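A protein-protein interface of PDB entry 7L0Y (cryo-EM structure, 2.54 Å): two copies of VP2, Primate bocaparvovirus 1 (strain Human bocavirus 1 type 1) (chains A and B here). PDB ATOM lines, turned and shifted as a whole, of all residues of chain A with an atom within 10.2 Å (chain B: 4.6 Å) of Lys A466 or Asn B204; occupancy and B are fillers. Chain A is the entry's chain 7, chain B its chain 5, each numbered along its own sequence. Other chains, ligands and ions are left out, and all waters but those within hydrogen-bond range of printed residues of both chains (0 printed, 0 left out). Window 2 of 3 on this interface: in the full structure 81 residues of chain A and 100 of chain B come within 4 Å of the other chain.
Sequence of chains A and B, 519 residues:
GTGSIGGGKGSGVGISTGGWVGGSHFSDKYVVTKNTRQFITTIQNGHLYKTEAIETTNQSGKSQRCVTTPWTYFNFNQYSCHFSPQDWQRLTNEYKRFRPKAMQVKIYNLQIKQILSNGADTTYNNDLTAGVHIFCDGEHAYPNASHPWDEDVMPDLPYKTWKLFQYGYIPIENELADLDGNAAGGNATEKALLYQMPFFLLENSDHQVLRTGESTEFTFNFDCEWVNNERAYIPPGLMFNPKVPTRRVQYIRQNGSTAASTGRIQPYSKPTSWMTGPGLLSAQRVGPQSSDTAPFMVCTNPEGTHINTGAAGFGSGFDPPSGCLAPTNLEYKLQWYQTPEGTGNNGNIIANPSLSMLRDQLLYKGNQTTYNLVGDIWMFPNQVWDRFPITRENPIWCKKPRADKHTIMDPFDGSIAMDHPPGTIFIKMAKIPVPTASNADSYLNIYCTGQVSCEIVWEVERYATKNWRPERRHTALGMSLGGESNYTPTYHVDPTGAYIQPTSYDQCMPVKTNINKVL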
ATOM      1  N   TYR A 233      32.711 -26.097   1.364  1.00  0.00           N
ATOM      2  CA  TYR A 233      32.249 -25.756   2.700  1.00  0.00           C
ATOM      3  C   TYR A 233      31.894 -26.981   3.524  1.00  0.00           C
ATOM      4  O   TYR A 233      31.858 -26.895   4.752  1.00  0.00           O
ATOM      5  CB  TYR A 233      31.053 -24.803   2.626  1.00  0.00           C
ATOM      6  CG  TYR A 233      29.829 -25.371   1.960  1.00  0.00           C
ATOM      7  CD1 TYR A 233      28.890 -26.082   2.684  1.00  0.00           C
ATOM      8  CD2 TYR A 233      29.597 -25.169   0.616  1.00  0.00           C
ATOM      9  CE1 TYR A 233      27.781 -26.592   2.090  1.00  0.00           C
ATOM     10  CE2 TYR A 233      28.485 -25.675   0.011  1.00  0.00           C
ATOM     11  CZ  TYR A 233      27.580 -26.387   0.751  1.00  0.00           C
ATOM     12  OH  TYR A 233      26.463 -26.896   0.141  1.00  0.00           O
ATOM     13  N   TYR A 463      32.975 -16.274 -10.994  1.00  0.00           N
ATOM     14  CA  TYR A 463      32.133 -17.162 -10.215  1.00  0.00           C
ATOM     15  C   TYR A 463      30.728 -16.591 -10.131  1.00  0.00           C
ATOM     16  O   TYR A 463      30.533 -15.379 -10.215  1.00  0.00           O
ATOM     17  CB  TYR A 463      32.695 -17.365  -8.807  1.00  0.00           C
ATOM     18  CG  TYR A 463      32.676 -16.117  -7.967  1.00  0.00           C
ATOM     19  CD1 TYR A 463      31.587 -15.812  -7.169  1.00  0.00           C
ATOM     20  CD2 TYR A 463      33.738 -15.236  -7.985  1.00  0.00           C
ATOM     21  CE1 TYR A 463      31.563 -14.677  -6.418  1.00  0.00           C
ATOM     22  CE2 TYR A 463      33.720 -14.100  -7.231  1.00  0.00           C
ATOM     23  CZ  TYR A 463      32.631 -13.824  -6.451  1.00  0.00           C
ATOM     24  OH  TYR A 463      32.612 -12.682  -5.699  1.00  0.00           O
ATOM     25  N   ALA A 464      29.757 -17.479  -9.990  1.00  0.00           N
ATOM     26  CA  ALA A 464      28.392 -17.123  -9.644  1.00  0.00           C
ATOM     27  C   ALA A 464      27.956 -18.043  -8.519  1.00  0.00           C
ATOM     28  O   ALA A 464      28.222 -19.245  -8.565  1.00  0.00           O
ATOM     29  CB  ALA A 464      27.459 -17.256 -10.844  1.00  0.00           C
ATOM     30  N   THR A 465      27.313 -17.486  -7.505  1.00  0.00           N
ATOM     31  CA  THR A 465      26.897 -18.288  -6.371  1.00  0.00           C
ATOM     32  C   THR A 465      25.470 -17.937  -5.993  1.00  0.00           C
ATOM     33  O   THR A 465      25.021 -16.804  -6.167  1.00  0.00           O
ATOM     34  CB  THR A 465      27.832 -18.100  -5.167  1.00  0.00           C
ATOM     35  OG1 THR A 465      27.518 -19.069  -4.161  1.00  0.00           O
ATOM     36  CG2 THR A 465      27.701 -16.710  -4.573  1.00  0.00           C
ATOM     37  N   LYS A 466      24.754 -18.934  -5.501  1.00  0.00           N
ATOM     38  CA  LYS A 466      23.447 -18.717  -4.913  1.00  0.00           C
ATOM     39  C   LYS A 466      23.539 -18.517  -3.414  1.00  0.00           C
ATOM     40  O   LYS A 466      22.508 -18.445  -2.747  1.00  0.00           O
ATOM     41  CB  LYS A 466      22.515 -19.889  -5.222  1.00  0.00           C
ATOM     42  CG  LYS A 466      22.419 -20.237  -6.680  1.00  0.00           C
ATOM     43  CD  LYS A 466      22.085 -19.052  -7.550  1.00  0.00           C
ATOM     44  CE  LYS A 466      20.658 -18.637  -7.408  1.00  0.00           C
ATOM     45  NZ  LYS A 466      20.298 -17.582  -8.383  1.00  0.00           N
ATOM     46  N   ASN A 467      24.747 -18.468  -2.875  1.00  0.00           N
ATOM     47  CA  ASN A 467      24.935 -18.237  -1.456  1.00  0.00           C
ATOM     48  C   ASN A 467      24.395 -16.875  -1.057  1.00  0.00           C
ATOM     49  O   ASN A 467      24.608 -15.878  -1.747  1.00  0.00           O
ATOM     50  CB  ASN A 467      26.410 -18.348  -1.101  1.00  0.00           C
ATOM     51  CG  ASN A 467      26.661 -18.242   0.374  1.00  0.00           C
ATOM     52  OD1 ASN A 467      25.801 -18.552   1.182  1.00  0.00           O
ATOM     53  ND2 ASN A 467      27.851 -17.813   0.733  1.00  0.00           N
ATOM     54  N   TRP A 468      23.686 -16.845   0.063  1.00  0.00           N
ATOM     55  CA  TRP A 468      23.074 -15.615   0.527  1.00  0.00           C
ATOM     56  C   TRP A 468      24.087 -14.737   1.242  1.00  0.00           C
ATOM     57  O   TRP A 468      24.033 -13.509   1.144  1.00  0.00           O
ATOM     58  CB  TRP A 468      21.908 -15.959   1.447  1.00  0.00           C
ATOM     59  CG  TRP A 468      21.189 -14.788   1.968  1.00  0.00           C
ATOM     60  CD1 TRP A 468      21.263 -14.280   3.216  1.00  0.00           C
ATOM     61  CD2 TRP A 468      20.284 -13.965   1.249  1.00  0.00           C
ATOM     62  NE1 TRP A 468      20.458 -13.192   3.327  1.00  0.00           N
ATOM     63  CE2 TRP A 468      19.841 -12.977   2.126  1.00  0.00           C
ATOM     64  CE3 TRP A 468      19.798 -13.974  -0.059  1.00  0.00           C
ATOM     65  CZ2 TRP A 468      18.939 -12.001   1.748  1.00  0.00           C
ATOM     66  CZ3 TRP A 468      18.907 -13.011  -0.432  1.00  0.00           C
ATOM     67  CH2 TRP A 468      18.484 -12.035   0.464  1.00  0.00           C
ATOM     68  N   ARG A 469      25.013 -15.349   1.943  1.00  0.00           N
ATOM     69  CA  ARG A 469      25.915 -14.727   2.890  1.00  0.00           C
ATOM     70  C   ARG A 469      27.196 -14.231   2.228  1.00  0.00           C
ATOM     71  O   ARG A 469      27.584 -14.712   1.164  1.00  0.00           O
ATOM     72  CB  ARG A 469      26.257 -15.709   3.994  1.00  0.00           C
ATOM     73  CG  ARG A 469      25.210 -15.812   5.045  1.00  0.00           C
ATOM     74  CD  ARG A 469      25.560 -16.865   6.044  1.00  0.00           C
ATOM     75  NE  ARG A 469      26.955 -16.748   6.444  1.00  0.00           N
ATOM     76  CZ  ARG A 469      27.426 -15.841   7.283  1.00  0.00           C
ATOM     77  NH1 ARG A 469      26.636 -14.928   7.800  1.00  0.00           N
ATOM     78  NH2 ARG A 469      28.707 -15.827   7.573  1.00  0.00           N
ATOM     79  N   PRO A 470      27.849 -13.246   2.839  1.00  0.00           N
ATOM     80  CA  PRO A 470      29.150 -12.785   2.338  1.00  0.00           C
ATOM     81  C   PRO A 470      30.209 -13.863   2.518  1.00  0.00           C
ATOM     82  O   PRO A 470      30.320 -14.470   3.580  1.00  0.00           O
ATOM     83  CB  PRO A 470      29.446 -11.556   3.201  1.00  0.00           C
ATOM     84  CG  PRO A 470      28.131 -11.119   3.683  1.00  0.00           C
ATOM     85  CD  PRO A 470      27.338 -12.359   3.894  1.00  0.00           C
ATOM     86  N   GLU A 471      30.944 -14.129   1.455  1.00  0.00           N
ATOM     87  CA  GLU A 471      32.050 -15.064   1.487  1.00  0.00           C
ATOM     88  C   GLU A 471      33.336 -14.404   1.977  1.00  0.00           C
ATOM     89  O   GLU A 471      33.500 -13.185   1.946  1.00  0.00           O
ATOM     90  CB  GLU A 471      32.227 -15.698   0.113  1.00  0.00           C
ATOM     91  CG  GLU A 471      31.138 -16.700  -0.199  1.00  0.00           C
ATOM     92  CD  GLU A 471      31.194 -17.256  -1.613  1.00  0.00           C
ATOM     93  OE1 GLU A 471      31.919 -16.703  -2.466  1.00  0.00           O
ATOM     94  OE2 GLU A 471      30.499 -18.261  -1.874  1.00  0.00           O
ATOM     95  N   ARG A 473      37.108 -13.212   1.850  1.00  0.00           N
ATOM     96  CA  ARG A 473      37.946 -12.617   0.823  1.00  0.00           C
ATOM     97  C   ARG A 473      39.326 -12.337   1.399  1.00  0.00           C
ATOM     98  O   ARG A 473      39.522 -12.336   2.613  1.00  0.00           O
ATOM     99  CB  ARG A 473      37.328 -11.328   0.276  1.00  0.00           C
ATOM    100  CG  ARG A 473      35.999 -11.537  -0.395  1.00  0.00           C
ATOM    101  CD  ARG A 473      36.199 -12.237  -1.700  1.00  0.00           C
ATOM    102  NE  ARG A 473      34.949 -12.577  -2.352  1.00  0.00           N
ATOM    103  CZ  ARG A 473      34.325 -13.737  -2.188  1.00  0.00           C
ATOM    104  NH1 ARG A 473      34.838 -14.654  -1.389  1.00  0.00           N
ATOM    105  NH2 ARG A 473      33.194 -13.983  -2.825  1.00  0.00           N
ATOM    106  N   ILE A 515      36.013 -18.497  -2.423  1.00  0.00           N
ATOM    107  CA  ILE A 515      34.792 -18.678  -3.193  1.00  0.00           C
ATOM    108  C   ILE A 515      34.245 -20.067  -2.914  1.00  0.00           C
ATOM    109  O   ILE A 515      34.924 -21.068  -3.146  1.00  0.00           O
ATOM    110  CB  ILE A 515      35.067 -18.482  -4.689  1.00  0.00           C
ATOM    111  CG1 ILE A 515      35.587 -17.064  -4.927  1.00  0.00           C
ATOM    112  CG2 ILE A 515      33.820 -18.734  -5.491  1.00  0.00           C
ATOM    113  CD1 ILE A 515      36.249 -16.864  -6.259  1.00  0.00           C
ATOM    114  N   ASN A 516      33.015 -20.136  -2.421  1.00  0.00           N
ATOM    115  CA  ASN A 516      32.416 -21.420  -2.103  1.00  0.00           C
ATOM    116  C   ASN A 516      31.868 -22.093  -3.353  1.00  0.00           C
ATOM    117  O   ASN A 516      31.374 -21.442  -4.273  1.00  0.00           O
ATOM    118  CB  ASN A 516      31.292 -21.256  -1.087  1.00  0.00           C
ATOM    119  CG  ASN A 516      31.795 -20.871   0.271  1.00  0.00           C
ATOM    120  OD1 ASN A 516      32.950 -21.108   0.600  1.00  0.00           O
ATOM    121  ND2 ASN A 516      30.931 -20.282   1.080  1.00  0.00           N
ATOM    122  N   LYS A 517      31.962 -23.414  -3.372  1.00  0.00           N
ATOM    123  CA  LYS A 517      31.317 -24.243  -4.375  1.00  0.00           C
ATOM    124  C   LYS A 517      30.394 -25.222  -3.667  1.00  0.00           C
ATOM    125  O   LYS A 517      30.650 -25.608  -2.525  1.00  0.00           O
ATOM    126  CB  LYS A 517      32.339 -24.989  -5.223  1.00  0.00           C
ATOM    127  CG  LYS A 517      33.229 -25.913  -4.431  1.00  0.00           C
ATOM    128  CD  LYS A 517      34.256 -26.569  -5.310  1.00  0.00           C
ATOM    129  CE  LYS A 517      35.208 -27.411  -4.498  1.00  0.00           C
ATOM    130  NZ  LYS A 517      36.219 -28.050  -5.365  1.00  0.00           N
ATOM    131  N   VAL A 518      29.330 -25.608  -4.353  1.00  0.00           N
ATOM    132  CA  VAL A 518      28.399 -26.583  -3.837  1.00  0.00           C
ATOM    133  C   VAL A 518      28.945 -27.899  -4.352  1.00  0.00           C
ATOM    134  O   VAL A 518      29.240 -28.023  -5.532  1.00  0.00           O
ATOM    135  CB  VAL A 518      26.974 -26.365  -4.388  1.00  0.00           C
ATOM    136  CG1 VAL A 518      26.102 -27.574  -4.104  1.00  0.00           C
ATOM    137  CG2 VAL A 518      26.353 -25.118  -3.793  1.00  0.00           C
ATOM    138  N   ALA B 141      23.225 -25.602  -8.391  1.00  0.00           N
ATOM    139  CA  ALA B 141      23.659 -24.393  -7.719  1.00  0.00           C
ATOM    140  C   ALA B 141      23.317 -24.395  -6.242  1.00  0.00           C
ATOM    141  O   ALA B 141      23.810 -23.545  -5.502  1.00  0.00           O
ATOM    142  CB  ALA B 141      23.030 -23.180  -8.399  1.00  0.00           C
ATOM    143  N   TYR B 142      22.499 -25.325  -5.806  1.00  0.00           N
ATOM    144  CA  TYR B 142      22.108 -25.469  -4.426  1.00  0.00           C
ATOM    145  C   TYR B 142      22.546 -26.822  -3.903  1.00  0.00           C
ATOM    146  O   TYR B 142      22.831 -27.733  -4.684  1.00  0.00           O
ATOM    147  CB  TYR B 142      20.590 -25.320  -4.282  1.00  0.00           C
ATOM    148  CG  TYR B 142      20.094 -23.940  -4.588  1.00  0.00           C
ATOM    149  CD1 TYR B 142      20.101 -22.958  -3.616  1.00  0.00           C
ATOM    150  CD2 TYR B 142      19.616 -23.613  -5.843  1.00  0.00           C
ATOM    151  CE1 TYR B 142      19.656 -21.703  -3.881  1.00  0.00           C
ATOM    152  CE2 TYR B 142      19.162 -22.357  -6.116  1.00  0.00           C
ATOM    153  CZ  TYR B 142      19.181 -21.403  -5.128  1.00  0.00           C
ATOM    154  OH  TYR B 142      18.734 -20.132  -5.377  1.00  0.00           O
ATOM    155  N   PHE B 199      24.697 -20.043   3.361  1.00  0.00           N
ATOM    156  CA  PHE B 199      23.269 -20.133   3.576  1.00  0.00           C
ATOM    157  C   PHE B 199      22.578 -20.028   2.235  1.00  0.00           C
ATOM    158  O   PHE B 199      22.913 -19.167   1.423  1.00  0.00           O
ATOM    159  CB  PHE B 199      22.794 -19.068   4.559  1.00  0.00           C
ATOM    160  CG  PHE B 199      21.324 -19.009   4.702  1.00  0.00           C
ATOM    161  CD1 PHE B 199      20.615 -20.143   5.019  1.00  0.00           C
ATOM    162  CD2 PHE B 199      20.661 -17.808   4.648  1.00  0.00           C
ATOM    163  CE1 PHE B 199      19.262 -20.097   5.159  1.00  0.00           C
ATOM    164  CE2 PHE B 199      19.310 -17.755   4.815  1.00  0.00           C
ATOM    165  CZ  PHE B 199      18.610 -18.903   5.075  1.00  0.00           C
ATOM    166  N   PHE B 200      21.650 -20.935   1.989  1.00  0.00           N
ATOM    167  CA  PHE B 200      21.004 -21.055   0.699  1.00  0.00           C
ATOM    168  C   PHE B 200      19.507 -20.882   0.851  1.00  0.00           C
ATOM    169  O   PHE B 200      18.875 -21.506   1.703  1.00  0.00           O
ATOM    170  CB  PHE B 200      21.315 -22.391   0.054  1.00  0.00           C
ATOM    171  CG  PHE B 200      22.750 -22.564  -0.276  1.00  0.00           C
ATOM    172  CD1 PHE B 200      23.263 -22.059  -1.449  1.00  0.00           C
ATOM    173  CD2 PHE B 200      23.594 -23.217   0.594  1.00  0.00           C
ATOM    174  CE1 PHE B 200      24.580 -22.210  -1.753  1.00  0.00           C
ATOM    175  CE2 PHE B 200      24.916 -23.370   0.291  1.00  0.00           C
ATOM    176  CZ  PHE B 200      25.411 -22.867  -0.883  1.00  0.00           C
ATOM    177  N   LEU B 201      18.970 -20.015   0.023  1.00  0.00           N
ATOM    178  CA  LEU B 201      17.555 -19.742  -0.082  1.00  0.00           C
ATOM    179  C   LEU B 201      17.152 -20.105  -1.490  1.00  0.00           C
ATOM    180  O   LEU B 201      17.785 -19.660  -2.446  1.00  0.00           O
ATOM    181  CB  LEU B 201      17.273 -18.272   0.165  1.00  0.00           C
ATOM    182  CG  LEU B 201      17.669 -17.796   1.544  1.00  0.00           C
ATOM    183  CD1 LEU B 201      17.624 -16.289   1.627  1.00  0.00           C
ATOM    184  CD2 LEU B 201      16.679 -18.394   2.471  1.00  0.00           C
ATOM    185  N   LEU B 202      16.111 -20.909  -1.633  1.00  0.00           N
ATOM    186  CA  LEU B 202      15.710 -21.235  -2.988  1.00  0.00           C
ATOM    187  C   LEU B 202      15.082 -20.036  -3.680  1.00  0.00           C
ATOM    188  O   LEU B 202      15.068 -19.985  -4.910  1.00  0.00           O
ATOM    189  CB  LEU B 202      14.759 -22.428  -2.997  1.00  0.00           C
ATOM    190  CG  LEU B 202      15.353 -23.821  -2.747  1.00  0.00           C
ATOM    191  CD1 LEU B 202      16.619 -23.987  -3.540  1.00  0.00           C
ATOM    192  CD2 LEU B 202      15.678 -24.018  -1.290  1.00  0.00           C
ATOM    193  N   GLU B 203      14.596 -19.060  -2.916  1.00  0.00           N
ATOM    194  CA  GLU B 203      13.986 -17.825  -3.398  1.00  0.00           C
ATOM    195  C   GLU B 203      14.958 -16.941  -4.140  1.00  0.00           C
ATOM    196  O   GLU B 203      14.543 -15.983  -4.790  1.00  0.00           O
ATOM    197  CB  GLU B 203      13.392 -17.066  -2.215  1.00  0.00           C
ATOM    198  CG  GLU B 203      12.176 -17.738  -1.600  1.00  0.00           C
ATOM    199  CD  GLU B 203      12.523 -18.933  -0.735  1.00  0.00           C
ATOM    200  OE1 GLU B 203      13.708 -19.295  -0.651  1.00  0.00           O
ATOM    201  OE2 GLU B 203      11.604 -19.523  -0.141  1.00  0.00           O
ATOM    202  N   ASN B 204      16.237 -17.251  -4.052  1.00  0.00           N
ATOM    203  CA  ASN B 204      17.309 -16.538  -4.717  1.00  0.00           C
ATOM    204  C   ASN B 204      17.352 -16.815  -6.213  1.00  0.00           C
ATOM    205  O   ASN B 204      18.235 -16.298  -6.895  1.00  0.00           O
ATOM    206  CB  ASN B 204      18.624 -16.935  -4.047  1.00  0.00           C
ATOM    207  CG  ASN B 204      19.716 -15.935  -4.263  1.00  0.00           C
ATOM    208  OD1 ASN B 204      19.462 -14.739  -4.388  1.00  0.00           O
ATOM    209  ND2 ASN B 204      20.947 -16.411  -4.293  1.00  0.00           N
ATOM    210  N   SER B 205      16.479 -17.667  -6.727  1.00  0.00           N
ATOM    211  CA  SER B 205      16.430 -17.988  -8.143  1.00  0.00           C
ATOM    212  C   SER B 205      15.017 -17.770  -8.678  1.00  0.00           C
ATOM    213  O   SER B 205      14.119 -17.334  -7.961  1.00  0.00           O
ATOM    214  CB  SER B 205      16.919 -19.419  -8.381  1.00  0.00           C
ATOM    215  OG  SER B 205      16.091 -20.369  -7.736  1.00  0.00           O
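OD1 of Asn A467 lies within hydrogen-bond range of N of Phe B199 (2.9 Å). O of Phe B199 sits at hydrogen-bond distance from N of Trp A468 (2.8 Å). O of Asn B204 lies within hydrogen-bond range of NZ of Lys A466 (2.8 Å).
The side-chain hydroxyl of Tyr B142 sits at hydrogen-bond distance from the backbone carbonyl oxygen of Leu B201 (3.1 Å). OG of Ser B205 sits at hydrogen-bond distance from O of Leu B202 (3.0 Å). OG1 of Thr A465 lies within hydrogen-bond range of N of Asn A467 (3.1 Å). ND2 of Asn A467 lies within hydrogen-bond range of O of Arg A469, 3.1 Å away.
Among the printed residues, pairs that only touch across the chains: Tyr A233 with Phe B200 (3.9 Å), Lys A466 with Ala B141 (3.5 Å), Lys A466 with Tyr B142 (3.2 Å), Lys A466 with Phe B200 (3.9 Å), Lys A466 with Ser B205 (3.8 Å), Asn A467 with Phe B200 (3.9 Å), Trp A468 with Leu B201 (3.6 Å), Arg A469 with Phe B199 (3.8 Å), Val A518 with Ala B141 (3.4 Å), Val A518 with Tyr B142 (3.3 Å) and Val A518 with Phe B200 (3.8 Å).
Of chain B, only Ala B141 (3.5 Å), Tyr B142 (3.2 Å), Phe B200 (3.9 Å), Asn B204 (2.8 Å) and Ser B205 (3.8 Å) come within 4 Å of Lys A466. Of chain A, only Lys A466 comes within 4 Å of Ser B205. Printed residues of chain B within 4 Å of Arg A469: Phe B199 (3.8 Å). Of the printed residues of chain A, Leu B201 touches Trp A468. Of the printed residues of chain B, Asn A467 touches Phe B199 (2.9 Å) and Phe B200 (3.9 Å). Of the printed residues of chain A, Phe B199 touches Asn A467 (2.9 Å), Trp A468 (2.8 Å) and Arg A469 (3.8 Å). The nearest residue of chain B that does not touch Lys A466 is Phe B199 (4.3 Å). The nearest residue of chain A that does not touch Asn B204 is Trp A468 (4.4 Å).
Of the 9 printed residues of chain B, 7 touch a printed residue of chain A. Hydrophobic or aromatic side chains of chain B that line the printed part of chain A: Ala B141, Tyr B142, Phe B199, Phe B200 and Leu B201. Of the 15 printed residues of chain A, 6 touch a printed residue of chain B. Printed residues of chain A that touch a printed residue of chain B: Tyr A233, Lys A466, Asn A467, Trp A468, Arg A469 and Val A518. Along chain A the printed residues that touch a printed residue of chain B span positions 233 to 518. Among the printed residues, 14 pairs touch across the chains.
No position is printed for both chains. Of the 14 pairs that touch across the chains among the printed residues, none has its exchanged pair printed and touching as well.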
